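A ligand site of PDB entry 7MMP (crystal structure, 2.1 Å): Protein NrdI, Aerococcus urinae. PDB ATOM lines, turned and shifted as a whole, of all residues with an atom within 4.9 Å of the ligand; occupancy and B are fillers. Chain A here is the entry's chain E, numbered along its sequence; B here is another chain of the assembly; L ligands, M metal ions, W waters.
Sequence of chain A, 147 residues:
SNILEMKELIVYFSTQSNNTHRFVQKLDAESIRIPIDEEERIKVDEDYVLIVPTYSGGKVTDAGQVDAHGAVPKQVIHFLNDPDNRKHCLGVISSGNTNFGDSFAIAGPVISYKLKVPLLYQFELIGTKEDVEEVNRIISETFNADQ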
ATOM      1  N   PHE A  13      19.931   6.522  -7.155  1.00  0.00           N
ATOM      2  CA  PHE A  13      21.317   6.341  -7.651  1.00  0.00           C
ATOM      3  C   PHE A  13      22.122   5.605  -6.586  1.00  0.00           C
ATOM      4  O   PHE A  13      21.894   5.825  -5.381  1.00  0.00           O
ATOM      5  CB  PHE A  13      21.984   7.678  -7.991  1.00  0.00           C
ATOM      6  CG  PHE A  13      23.415   7.526  -8.423  1.00  0.00           C
ATOM      7  CD1 PHE A  13      23.728   7.254  -9.745  1.00  0.00           C
ATOM      8  CD2 PHE A  13      24.442   7.595  -7.497  1.00  0.00           C
ATOM      9  CE1 PHE A  13      25.043   7.089 -10.141  1.00  0.00           C
ATOM     10  CE2 PHE A  13      25.756   7.430  -7.894  1.00  0.00           C
ATOM     11  CZ  PHE A  13      26.060   7.179  -9.213  1.00  0.00           C
ATOM     12  N   SER A  14      23.044   4.759  -7.046  1.00  0.00           N
ATOM     13  CA  SER A  14      23.956   3.956  -6.199  1.00  0.00           C
ATOM     14  C   SER A  14      25.241   3.725  -6.998  1.00  0.00           C
ATOM     15  O   SER A  14      25.133   3.322  -8.161  1.00  0.00           O
ATOM     16  CB  SER A  14      23.296   2.644  -5.798  1.00  0.00           C
ATOM     17  OG  SER A  14      23.969   2.031  -4.710  1.00  0.00           O
ATOM     18  N   THR A  15      26.396   4.005  -6.405  1.00  0.00           N
ATOM     19  CA  THR A  15      27.712   3.705  -7.024  1.00  0.00           C
ATOM     20  C   THR A  15      27.908   2.184  -7.008  1.00  0.00           C
ATOM     21  O   THR A  15      26.958   1.467  -6.600  1.00  0.00           O
ATOM     22  CB  THR A  15      28.871   4.446  -6.325  1.00  0.00           C
ATOM     23  OG1 THR A  15      29.069   3.855  -5.038  1.00  0.00           O
ATOM     24  CG2 THR A  15      28.641   5.941  -6.200  1.00  0.00           C
ATOM     25  N   SER A  17      29.490   0.437  -4.992  1.00  0.00           N
ATOM     26  CA  SER A  17      29.457  -0.068  -3.591  1.00  0.00           C
ATOM     27  C   SER A  17      28.035  -0.544  -3.214  1.00  0.00           C
ATOM     28  O   SER A  17      27.933  -1.399  -2.309  1.00  0.00           O
ATOM     29  CB  SER A  17      30.002   0.936  -2.603  1.00  0.00           C
ATOM     30  OG  SER A  17      29.553   2.254  -2.872  1.00  0.00           O
ATOM     31  N   ASN A  18      26.998   0.009  -3.862  1.00  0.00           N
ATOM     32  CA  ASN A  18      25.617  -0.540  -3.870  1.00  0.00           C
ATOM     33  C   ASN A  18      24.954  -0.437  -2.479  1.00  0.00           C
ATOM     34  O   ASN A  18      24.033  -1.243  -2.233  1.00  0.00           O
ATOM     35  CB  ASN A  18      25.595  -1.988  -4.373  1.00  0.00           C
ATOM     36  CG  ASN A  18      25.662  -2.059  -5.887  1.00  0.00           C
ATOM     37  OD1 ASN A  18      24.903  -1.374  -6.563  1.00  0.00           O
ATOM     38  ND2 ASN A  18      26.561  -2.875  -6.398  1.00  0.00           N
ATOM     39  N   ASN A  19      25.367   0.510  -1.633  1.00  0.00           N
ATOM     40  CA  ASN A  19      24.721   0.741  -0.309  1.00  0.00           C
ATOM     41  C   ASN A  19      23.273   1.199  -0.511  1.00  0.00           C
ATOM     42  O   ASN A  19      22.363   0.603   0.105  1.00  0.00           O
ATOM     43  CB  ASN A  19      25.473   1.761   0.544  1.00  0.00           C
ATOM     44  CG  ASN A  19      26.775   1.253   1.140  1.00  0.00           C
ATOM     45  OD1 ASN A  19      27.188   0.118   0.894  1.00  0.00           O
ATOM     46  ND2 ASN A  19      27.426   2.101   1.921  1.00  0.00           N
ATOM     47  N   THR A  20      23.078   2.244  -1.319  1.00  0.00           N
ATOM     48  CA  THR A  20      21.757   2.860  -1.591  1.00  0.00           C
ATOM     49  C   THR A  20      20.889   1.850  -2.354  1.00  0.00           C
ATOM     50  O   THR A  20      19.677   1.769  -2.066  1.00  0.00           O
ATOM     51  CB  THR A  20      21.884   4.187  -2.355  1.00  0.00           C
ATOM     52  OG1 THR A  20      22.951   4.950  -1.788  1.00  0.00           O
ATOM     53  CG2 THR A  20      20.612   4.992  -2.327  1.00  0.00           C
ATOM     54  N   HIS A  21      21.486   1.107  -3.278  1.00  0.00           N
ATOM     55  CA  HIS A  21      20.817   0.001  -4.011  1.00  0.00           C
ATOM     56  C   HIS A  21      20.193  -0.971  -3.014  1.00  0.00           C
ATOM     57  O   HIS A  21      18.997  -1.273  -3.158  1.00  0.00           O
ATOM     58  CB  HIS A  21      21.779  -0.706  -4.975  1.00  0.00           C
ATOM     59  CG  HIS A  21      21.195  -1.927  -5.588  1.00  0.00           C
ATOM     60  ND1 HIS A  21      20.186  -1.868  -6.535  1.00  0.00           N
ATOM     61  CD2 HIS A  21      21.449  -3.236  -5.397  1.00  0.00           C
ATOM     62  CE1 HIS A  21      19.856  -3.084  -6.882  1.00  0.00           C
ATOM     63  NE2 HIS A  21      20.618  -3.939  -6.208  1.00  0.00           N
ATOM     64  N   PRO A  53      22.784   8.920  -2.510  1.00  0.00           N
ATOM     65  CA  PRO A  53      23.878   9.143  -1.576  1.00  0.00           C
ATOM     66  C   PRO A  53      24.627  10.455  -1.837  1.00  0.00           C
ATOM     67  O   PRO A  53      24.424  11.056  -2.887  1.00  0.00           O
ATOM     68  CB  PRO A  53      24.781   7.930  -1.862  1.00  0.00           C
ATOM     69  CG  PRO A  53      24.636   7.751  -3.359  1.00  0.00           C
ATOM     70  CD  PRO A  53      23.181   8.063  -3.631  1.00  0.00           C
ATOM     71  N   THR A  54      25.498  10.838  -0.903  1.00  0.00           N
ATOM     72  CA  THR A  54      26.269  12.105  -0.901  1.00  0.00           C
ATOM     73  C   THR A  54      27.750  11.797  -1.118  1.00  0.00           C
ATOM     74  O   THR A  54      28.254  10.823  -0.515  1.00  0.00           O
ATOM     75  CB  THR A  54      26.024  12.854   0.418  1.00  0.00           C
ATOM     76  OG1 THR A  54      24.606  12.958   0.589  1.00  0.00           O
ATOM     77  CG2 THR A  54      26.671  14.214   0.430  1.00  0.00           C
ATOM     78  N   TYR A  55      28.440  12.606  -1.933  1.00  0.00           N
ATOM     79  CA  TYR A  55      29.850  12.376  -2.350  1.00  0.00           C
ATOM     80  C   TYR A  55      30.643  13.688  -2.382  1.00  0.00           C
ATOM     81  O   TYR A  55      31.626  13.786  -3.147  1.00  0.00           O
ATOM     82  CB  TYR A  55      29.847  11.621  -3.690  1.00  0.00           C
ATOM     83  CG  TYR A  55      29.691  10.137  -3.503  1.00  0.00           C
ATOM     84  CD1 TYR A  55      30.781   9.367  -3.133  1.00  0.00           C
ATOM     85  CD2 TYR A  55      28.463   9.510  -3.632  1.00  0.00           C
ATOM     86  CE1 TYR A  55      30.668   8.002  -2.924  1.00  0.00           C
ATOM     87  CE2 TYR A  55      28.335   8.140  -3.434  1.00  0.00           C
ATOM     88  CZ  TYR A  55      29.443   7.381  -3.076  1.00  0.00           C
ATOM     89  OH  TYR A  55      29.350   6.036  -2.867  1.00  0.00           O
ATOM     90  N   SER A  56      30.285  14.658  -1.535  1.00  0.00           N
ATOM     91  CA  SER A  56      31.055  15.927  -1.364  1.00  0.00           C
ATOM     92  C   SER A  56      32.384  15.627  -0.653  1.00  0.00           C
ATOM     93  O   SER A  56      33.358  16.340  -0.936  1.00  0.00           O
ATOM     94  CB  SER A  56      30.245  16.966  -0.654  1.00  0.00           C
ATOM     95  OG  SER A  56      29.921  16.552   0.666  1.00  0.00           O
ATOM     96  N   GLY A  57      32.424  14.630   0.226  1.00  0.00           N
ATOM     97  CA  GLY A  57      33.657  14.164   0.888  1.00  0.00           C
ATOM     98  C   GLY A  57      34.084  15.076   2.037  1.00  0.00           C
ATOM     99  O   GLY A  57      35.253  14.965   2.452  1.00  0.00           O
ATOM    100  N   GLY A  58      33.175  15.930   2.525  1.00  0.00           N
ATOM    101  CA  GLY A  58      33.393  16.783   3.715  1.00  0.00           C
ATOM    102  C   GLY A  58      34.331  17.937   3.427  1.00  0.00           C
ATOM    103  O   GLY A  58      35.009  18.372   4.378  1.00  0.00           O
ATOM    104  N   SER A  95      21.248  10.021   1.610  1.00  0.00           N
ATOM    105  CA  SER A  95      22.027   9.152   2.520  1.00  0.00           C
ATOM    106  C   SER A  95      23.487   9.615   2.555  1.00  0.00           C
ATOM    107  O   SER A  95      23.896  10.442   1.732  1.00  0.00           O
ATOM    108  CB  SER A  95      21.931   7.713   2.122  1.00  0.00           C
ATOM    109  OG  SER A  95      22.582   7.503   0.884  1.00  0.00           O
ATOM    110  N   GLY A  96      24.226   9.036   3.491  1.00  0.00           N
ATOM    111  CA  GLY A  96      25.666   9.250   3.690  1.00  0.00           C
ATOM    112  C   GLY A  96      26.103   8.625   4.997  1.00  0.00           C
ATOM    113  O   GLY A  96      25.633   7.507   5.299  1.00  0.00           O
ATOM    114  N   ASN A  97      26.927   9.341   5.759  1.00  0.00           N
ATOM    115  CA  ASN A  97      27.503   8.884   7.043  1.00  0.00           C
ATOM    116  C   ASN A  97      27.712  10.112   7.923  1.00  0.00           C
ATOM    117  O   ASN A  97      28.392  11.044   7.465  1.00  0.00           O
ATOM    118  CB  ASN A  97      28.801   8.100   6.804  1.00  0.00           C
ATOM    119  CG  ASN A  97      29.249   7.307   8.010  1.00  0.00           C
ATOM    120  OD1 ASN A  97      29.346   7.846   9.103  1.00  0.00           O
ATOM    121  ND2 ASN A  97      29.564   6.032   7.804  1.00  0.00           N
ATOM    122  N   PHE A 100      30.880  12.328   8.391  1.00  0.00           N
ATOM    123  CA  PHE A 100      31.181  13.486   7.507  1.00  0.00           C
ATOM    124  C   PHE A 100      30.680  14.791   8.134  1.00  0.00           C
ATOM    125  O   PHE A 100      30.854  15.861   7.505  1.00  0.00           O
ATOM    126  CB  PHE A 100      30.586  13.269   6.109  1.00  0.00           C
ATOM    127  CG  PHE A 100      31.420  12.357   5.256  1.00  0.00           C
ATOM    128  CD1 PHE A 100      32.571  12.835   4.646  1.00  0.00           C
ATOM    129  CD2 PHE A 100      31.082  11.031   5.091  1.00  0.00           C
ATOM    130  CE1 PHE A 100      33.357  11.994   3.868  1.00  0.00           C
ATOM    131  CE2 PHE A 100      31.868  10.191   4.313  1.00  0.00           C
ATOM    132  CZ  PHE A 100      33.005  10.672   3.702  1.00  0.00           C
ATOM    133  N   SER A 103      28.703  17.836   6.532  1.00  0.00           N
ATOM    134  CA  SER A 103      28.463  17.399   5.131  1.00  0.00           C
ATOM    135  C   SER A 103      27.617  16.116   5.115  1.00  0.00           C
ATOM    136  O   SER A 103      27.438  15.568   4.012  1.00  0.00           O
ATOM    137  CB  SER A 103      29.752  17.237   4.394  1.00  0.00           C
ATOM    138  OG  SER A 103      30.436  18.476   4.318  1.00  0.00           O
ATOM    139  N   PHE A 104      27.101  15.662   6.258  1.00  0.00           N
ATOM    140  CA  PHE A 104      26.243  14.456   6.336  1.00  0.00           C
ATOM    141  C   PHE A 104      25.004  14.635   5.436  1.00  0.00           C
ATOM    142  O   PHE A 104      24.238  15.580   5.666  1.00  0.00           O
ATOM    143  CB  PHE A 104      25.802  14.145   7.769  1.00  0.00           C
ATOM    144  CG  PHE A 104      24.692  13.125   7.820  1.00  0.00           C
ATOM    145  CD1 PHE A 104      24.842  11.887   7.215  1.00  0.00           C
ATOM    146  CD2 PHE A 104      23.493  13.400   8.455  1.00  0.00           C
ATOM    147  CE1 PHE A 104      23.829  10.949   7.238  1.00  0.00           C
ATOM    148  CE2 PHE A 104      22.466  12.465   8.477  1.00  0.00           C
ATOM    149  CZ  PHE A 104      22.634  11.241   7.877  1.00  0.00           C
ATOM    150  N   ALA A 105      24.857  13.755   4.440  1.00  0.00           N
ATOM    151  CA  ALA A 105      23.642  13.558   3.612  1.00  0.00           C
ATOM    152  C   ALA A 105      23.250  14.828   2.840  1.00  0.00           C
ATOM    153  O   ALA A 105      22.080  14.898   2.395  1.00  0.00           O
ATOM    154  CB  ALA A 105      22.499  13.098   4.489  1.00  0.00           C
ATOM    155  N   LEU A 125      24.195   4.498   4.878  1.00  0.00           N
ATOM    156  CA  LEU A 125      24.698   3.206   4.343  1.00  0.00           C
ATOM    157  C   LEU A 125      23.516   2.398   3.791  1.00  0.00           C
ATOM    158  O   LEU A 125      22.847   2.919   2.879  1.00  0.00           O
ATOM    159  CB  LEU A 125      25.464   2.483   5.467  1.00  0.00           C
ATOM    160  CG  LEU A 125      26.548   3.326   6.142  1.00  0.00           C
ATOM    161  CD1 LEU A 125      27.235   2.541   7.246  1.00  0.00           C
ATOM    162  CD2 LEU A 125      27.566   3.821   5.137  1.00  0.00           C
ATOM    163  N   LYS B  41      35.869   3.165  -8.237  1.00  0.00           N
ATOM    164  CA  LYS B  41      35.733   3.410  -6.772  1.00  0.00           C
ATOM    165  C   LYS B  41      37.115   3.717  -6.174  1.00  0.00           C
ATOM    166  O   LYS B  41      37.188   4.602  -5.307  1.00  0.00           O
ATOM    167  CB  LYS B  41      35.028   2.218  -6.120  1.00  0.00           C
ATOM    168  CG  LYS B  41      34.759   2.357  -4.622  1.00  0.00           C
ATOM    169  CD  LYS B  41      33.944   3.569  -4.242  1.00  0.00           C
ATOM    170  CE  LYS B  41      32.522   3.547  -4.744  1.00  0.00           C
ATOM    171  NZ  LYS B  41      31.659   4.482  -3.983  1.00  0.00           N
ATOM    172  N   GLU B  44      37.852   7.421  -7.097  1.00  0.00           N
ATOM    173  CA  GLU B  44      36.954   8.228  -6.229  1.00  0.00           C
ATOM    174  C   GLU B  44      37.596   8.369  -4.836  1.00  0.00           C
ATOM    175  O   GLU B  44      37.718   9.510  -4.341  1.00  0.00           O
ATOM    176  CB  GLU B  44      35.573   7.571  -6.218  1.00  0.00           C
ATOM    177  CG  GLU B  44      34.509   8.282  -5.395  1.00  0.00           C
ATOM    178  CD  GLU B  44      33.075   7.930  -5.787  1.00  0.00           C
ATOM    179  OE1 GLU B  44      32.355   8.846  -6.274  1.00  0.00           O
ATOM    180  OE2 GLU B  44      32.662   6.740  -5.589  1.00  0.00           O
ATOM    181  N   VAL B  45      38.031   7.264  -4.233  1.00  0.00           N
ATOM    182  CA  VAL B  45      38.592   7.255  -2.849  1.00  0.00           C
ATOM    183  C   VAL B  45      39.968   7.927  -2.845  1.00  0.00           C
ATOM    184  O   VAL B  45      40.204   8.743  -1.947  1.00  0.00           O
ATOM    185  CB  VAL B  45      38.640   5.824  -2.271  1.00  0.00           C
ATOM    186  CG1 VAL B  45      39.455   5.738  -0.984  1.00  0.00           C
ATOM    187  CG2 VAL B  45      37.234   5.296  -2.038  1.00  0.00           C
ATOM    188  N   ARG B  48      39.702  11.748  -3.065  1.00  0.00           N
ATOM    189  CA  ARG B  48      39.095  12.361  -1.845  1.00  0.00           C
ATOM    190  C   ARG B  48      40.127  12.380  -0.715  1.00  0.00           C
ATOM    191  O   ARG B  48      40.326  13.461  -0.120  1.00  0.00           O
ATOM    192  CB  ARG B  48      37.788  11.645  -1.461  1.00  0.00           C
ATOM    193  CG  ARG B  48      37.078  12.248  -0.258  1.00  0.00           C
ATOM    194  CD  ARG B  48      37.063  13.774  -0.234  1.00  0.00           C
ATOM    195  NE  ARG B  48      36.675  14.374  -1.505  1.00  0.00           N
ATOM    196  CZ  ARG B  48      36.984  15.604  -1.896  1.00  0.00           C
ATOM    197  NH1 ARG B  48      37.669  16.418  -1.108  1.00  0.00           N
ATOM    198  NH2 ARG B  48      36.576  16.041  -3.078  1.00  0.00           N
ATOM    199  N   ILE B 217      36.058   7.046   5.615  1.00  0.00           N
ATOM    200  CA  ILE B 217      36.463   6.515   4.273  1.00  0.00           C
ATOM    201  C   ILE B 217      37.308   5.248   4.438  1.00  0.00           C
ATOM    202  O   ILE B 217      37.108   4.324   3.649  1.00  0.00           O
ATOM    203  CB  ILE B 217      37.195   7.600   3.438  1.00  0.00           C
ATOM    204  CG1 ILE B 217      36.250   8.767   3.127  1.00  0.00           C
ATOM    205  CG2 ILE B 217      37.783   6.983   2.176  1.00  0.00           C
ATOM    206  CD1 ILE B 217      36.859   9.852   2.278  1.00  0.00           C
ATOM    207  N   PHE B 220      34.862   2.471   5.223  1.00  0.00           N
ATOM    208  CA  PHE B 220      34.055   2.235   4.000  1.00  0.00           C
ATOM    209  C   PHE B 220      34.864   1.379   3.016  1.00  0.00           C
ATOM    210  O   PHE B 220      34.339   0.375   2.508  1.00  0.00           O
ATOM    211  CB  PHE B 220      33.642   3.530   3.293  1.00  0.00           C
ATOM    212  CG  PHE B 220      33.193   3.278   1.879  1.00  0.00           C
ATOM    213  CD1 PHE B 220      31.894   2.871   1.614  1.00  0.00           C
ATOM    214  CD2 PHE B 220      34.083   3.360   0.818  1.00  0.00           C
ATOM    215  CE1 PHE B 220      31.494   2.588   0.306  1.00  0.00           C
ATOM    216  CE2 PHE B 220      33.688   3.072  -0.477  1.00  0.00           C
ATOM    217  CZ  PHE B 220      32.390   2.675  -0.732  1.00  0.00           C
ATOM    218  N   ASN B 287      28.792  -1.535   6.537  1.00  0.00           N
ATOM    219  CA  ASN B 287      29.840  -1.309   5.509  1.00  0.00           C
ATOM    220  C   ASN B 287      30.584  -2.625   5.219  1.00  0.00           C
ATOM    221  O   ASN B 287      31.404  -2.605   4.278  1.00  0.00           O
ATOM    222  CB  ASN B 287      30.764  -0.140   5.871  1.00  0.00           C
ATOM    223  CG  ASN B 287      30.360   1.135   5.161  1.00  0.00           C
ATOM    224  OD1 ASN B 287      29.525   1.105   4.243  1.00  0.00           O
ATOM    225  ND2 ASN B 287      30.939   2.248   5.549  1.00  0.00           N
HETATM  226  N1  LIG L   1      28.537  10.730   3.112  1.00  0.00           N
HETATM  227  C1  LIG L   1      28.050  11.937   3.484  1.00  0.00           C
HETATM  228  O1  LIG L   1      27.059  11.956   4.252  1.00  0.00           O
HETATM  229  N2  LIG L   1      28.581  13.106   3.063  1.00  0.00           N
HETATM  230  C2  LIG L   1      29.649  13.147   2.251  1.00  0.00           C
HETATM  231  O2  LIG L   1      30.121  14.248   1.887  1.00  0.00           O
HETATM  232  C3  LIG L   1      30.241  11.862   1.803  1.00  0.00           C
HETATM  233  N3  LIG L   1      31.309  11.813   0.985  1.00  0.00           N
HETATM  234  C4  LIG L   1      31.841  10.631   0.595  1.00  0.00           C
HETATM  235  C5  LIG L   1      32.946  10.634  -0.244  1.00  0.00           C
HETATM  236  C6  LIG L   1      33.511   9.427  -0.664  1.00  0.00           C
HETATM  237  C7  LIG L   1      34.712   9.461  -1.571  1.00  0.00           C
HETATM  238  C8  LIG L   1      32.930   8.131  -0.201  1.00  0.00           C
HETATM  239  C9  LIG L   1      33.521   6.819  -0.635  1.00  0.00           C
HETATM  240  C10 LIG L   1      31.827   8.136   0.632  1.00  0.00           C
HETATM  241  C11 LIG L   1      31.246   9.339   1.057  1.00  0.00           C
HETATM  242  N4  LIG L   1      30.119   9.368   1.908  1.00  0.00           N
HETATM  243  C12 LIG L   1      29.599  10.627   2.295  1.00  0.00           C
HETATM  244  C13 LIG L   1      29.473   8.147   2.398  1.00  0.00           C
HETATM  245  C14 LIG L   1      28.587   7.552   1.302  1.00  0.00           C
HETATM  246  O3  LIG L   1      27.567   8.469   0.890  1.00  0.00           O
HETATM  247  C15 LIG L   1      27.978   6.246   1.805  1.00  0.00           C
HETATM  248  O4  LIG L   1      29.014   5.261   1.861  1.00  0.00           O
HETATM  249  C16 LIG L   1      26.806   5.747   0.953  1.00  0.00           C
HETATM  250  O5  LIG L   1      26.118   4.712   1.692  1.00  0.00           O
HETATM  251  C17 LIG L   1      27.290   5.207  -0.400  1.00  0.00           C
HETATM  252  O6  LIG L   1      26.182   4.874  -1.245  1.00  0.00           O
HETATM  253  P1  LIG L   1      26.344   3.968  -2.568  1.00  0.00           P
HETATM  254  O7  LIG L   1      27.098   2.740  -2.104  1.00  0.00           O
HETATM  255  O8  LIG L   1      24.917   3.698  -2.975  1.00  0.00           O
HETATM  256  O9  LIG L   1      27.107   4.835  -3.537  1.00  0.00           O
HETATM  257 CA    CA M   1      30.643   5.533   4.537  1.00  0.00          CA
HETATM  258  O   HOH W   1      23.451   4.766   1.089  1.00  0.00           O
HETATM  259  O   HOH W   2      33.226   7.130   3.371  1.00  0.00           O
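An oxygen (O9) of the ligand is in hydrogen-bond range of the backbone NH (N) of Thr 15. The side-chain hydroxyl (OG1) of Thr 15 sits at hydrogen-bond distance from an oxygen (O9) of the ligand. An oxygen (O7) of the ligand is in hydrogen-bond range of the side-chain hydroxyl of Ser 17 (2.6 Å). OG of Ser 56 is in hydrogen-bond range of O2 of the ligand (2.6 Å). O1 of the ligand sits at hydrogen-bond distance from N of Asn 97, 3.0 Å away. N2 of the ligand is in hydrogen-bond range of O of Ser 103, at 2.9 Å. The backbone NH of Ala 105 is in hydrogen-bond range of an oxygen (O1) of the ligand (2.8 Å). The side-chain amide nitrogen (ND2) of Asn 19 sits at hydrogen-bond distance from an oxygen (O5) of the ligand (2.9 Å). An oxygen (O8) of the ligand is in hydrogen-bond range of the side-chain hydroxyl of Thr 20 (2.6 Å). N of Thr 20 is in hydrogen-bond range of O8 of the ligand, at 2.9 Å. An oxygen (O2) of the ligand sits at hydrogen-bond distance from the backbone NH of Ser 56 (3.5 Å). The side-chain hydroxyl of Tyr 55 is in hydrogen-bond range of an oxygen (O9) of the ligand (2.6 Å). N of Gly 57 is in hydrogen-bond range of O2 of the ligand (2.9 Å). The backbone NH (N) of Asn 19 lies within hydrogen-bond range of an oxygen (O7) of the ligand. An oxygen (O7) of the ligand lies within hydrogen-bond range of the backbone NH (N) of Asn 18 (3.2 Å). The side-chain hydroxyl (OG) of Ser 14 is in hydrogen-bond range of an oxygen (O8) of the ligand (2.6 Å). The backbone carbonyl oxygen (O) of Thr 54 is in hydrogen-bond range of an oxygen (O3) of the ligand (2.8 Å).
The side-chain amino group (NZ) of Lys 41 of chain B lies within hydrogen-bond range of the side-chain hydroxyl (OH) of Tyr 55, 3.0 Å away. OG of Ser 17 sits at hydrogen-bond distance from OG1 of Thr 15 (2.7 Å). The side-chain hydroxyl (OG1) of Thr 15 is in hydrogen-bond range of the side-chain amino group (NZ) of Lys 41 of chain B (2.9 Å). The side-chain amide nitrogen (ND2) of Asn 19 is in hydrogen-bond range of the side-chain amide oxygen (OD1) of Asn 287 of chain B (3.3 Å). The backbone carbonyl oxygen (O) of Ser 95 is in hydrogen-bond range of the side-chain hydroxyl (OG1) of Thr 54 (2.9 Å). OH of Tyr 55 lies within hydrogen-bond range of OG1 of Thr 15 (3.1 Å). The backbone NH of Leu 125 sits at hydrogen-bond distance from the backbone carbonyl oxygen of Gly 96, 3.4 Å away. OG of Ser 14 sits at hydrogen-bond distance from N of His 21 (3.0 Å).
Residues that only touch the ligand: Phe 100 (3.1 Å), Gly 96 (3.1 Å), Phe 104 (3.4 Å), Leu 125 (3.4 Å), Pro 53 (3.4 Å), Gly 58 (3.5 Å), Phe 220 of chain B (3.8 Å) and Arg 48 of chain B (3.8 Å). Of the 29 residues printed, 21 come within 4 Å of the ligand. The nearest printed residue that does not touch the ligand is Glu 44 of chain B (4.01 Å).
Water W1 lies within hydrogen-bond range of O of Leu 125 (2.6 Å), O5 of the ligand (2.7 Å), OG of Ser 95 (2.9 Å) and OG1 of Thr 20 (2.9 Å).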
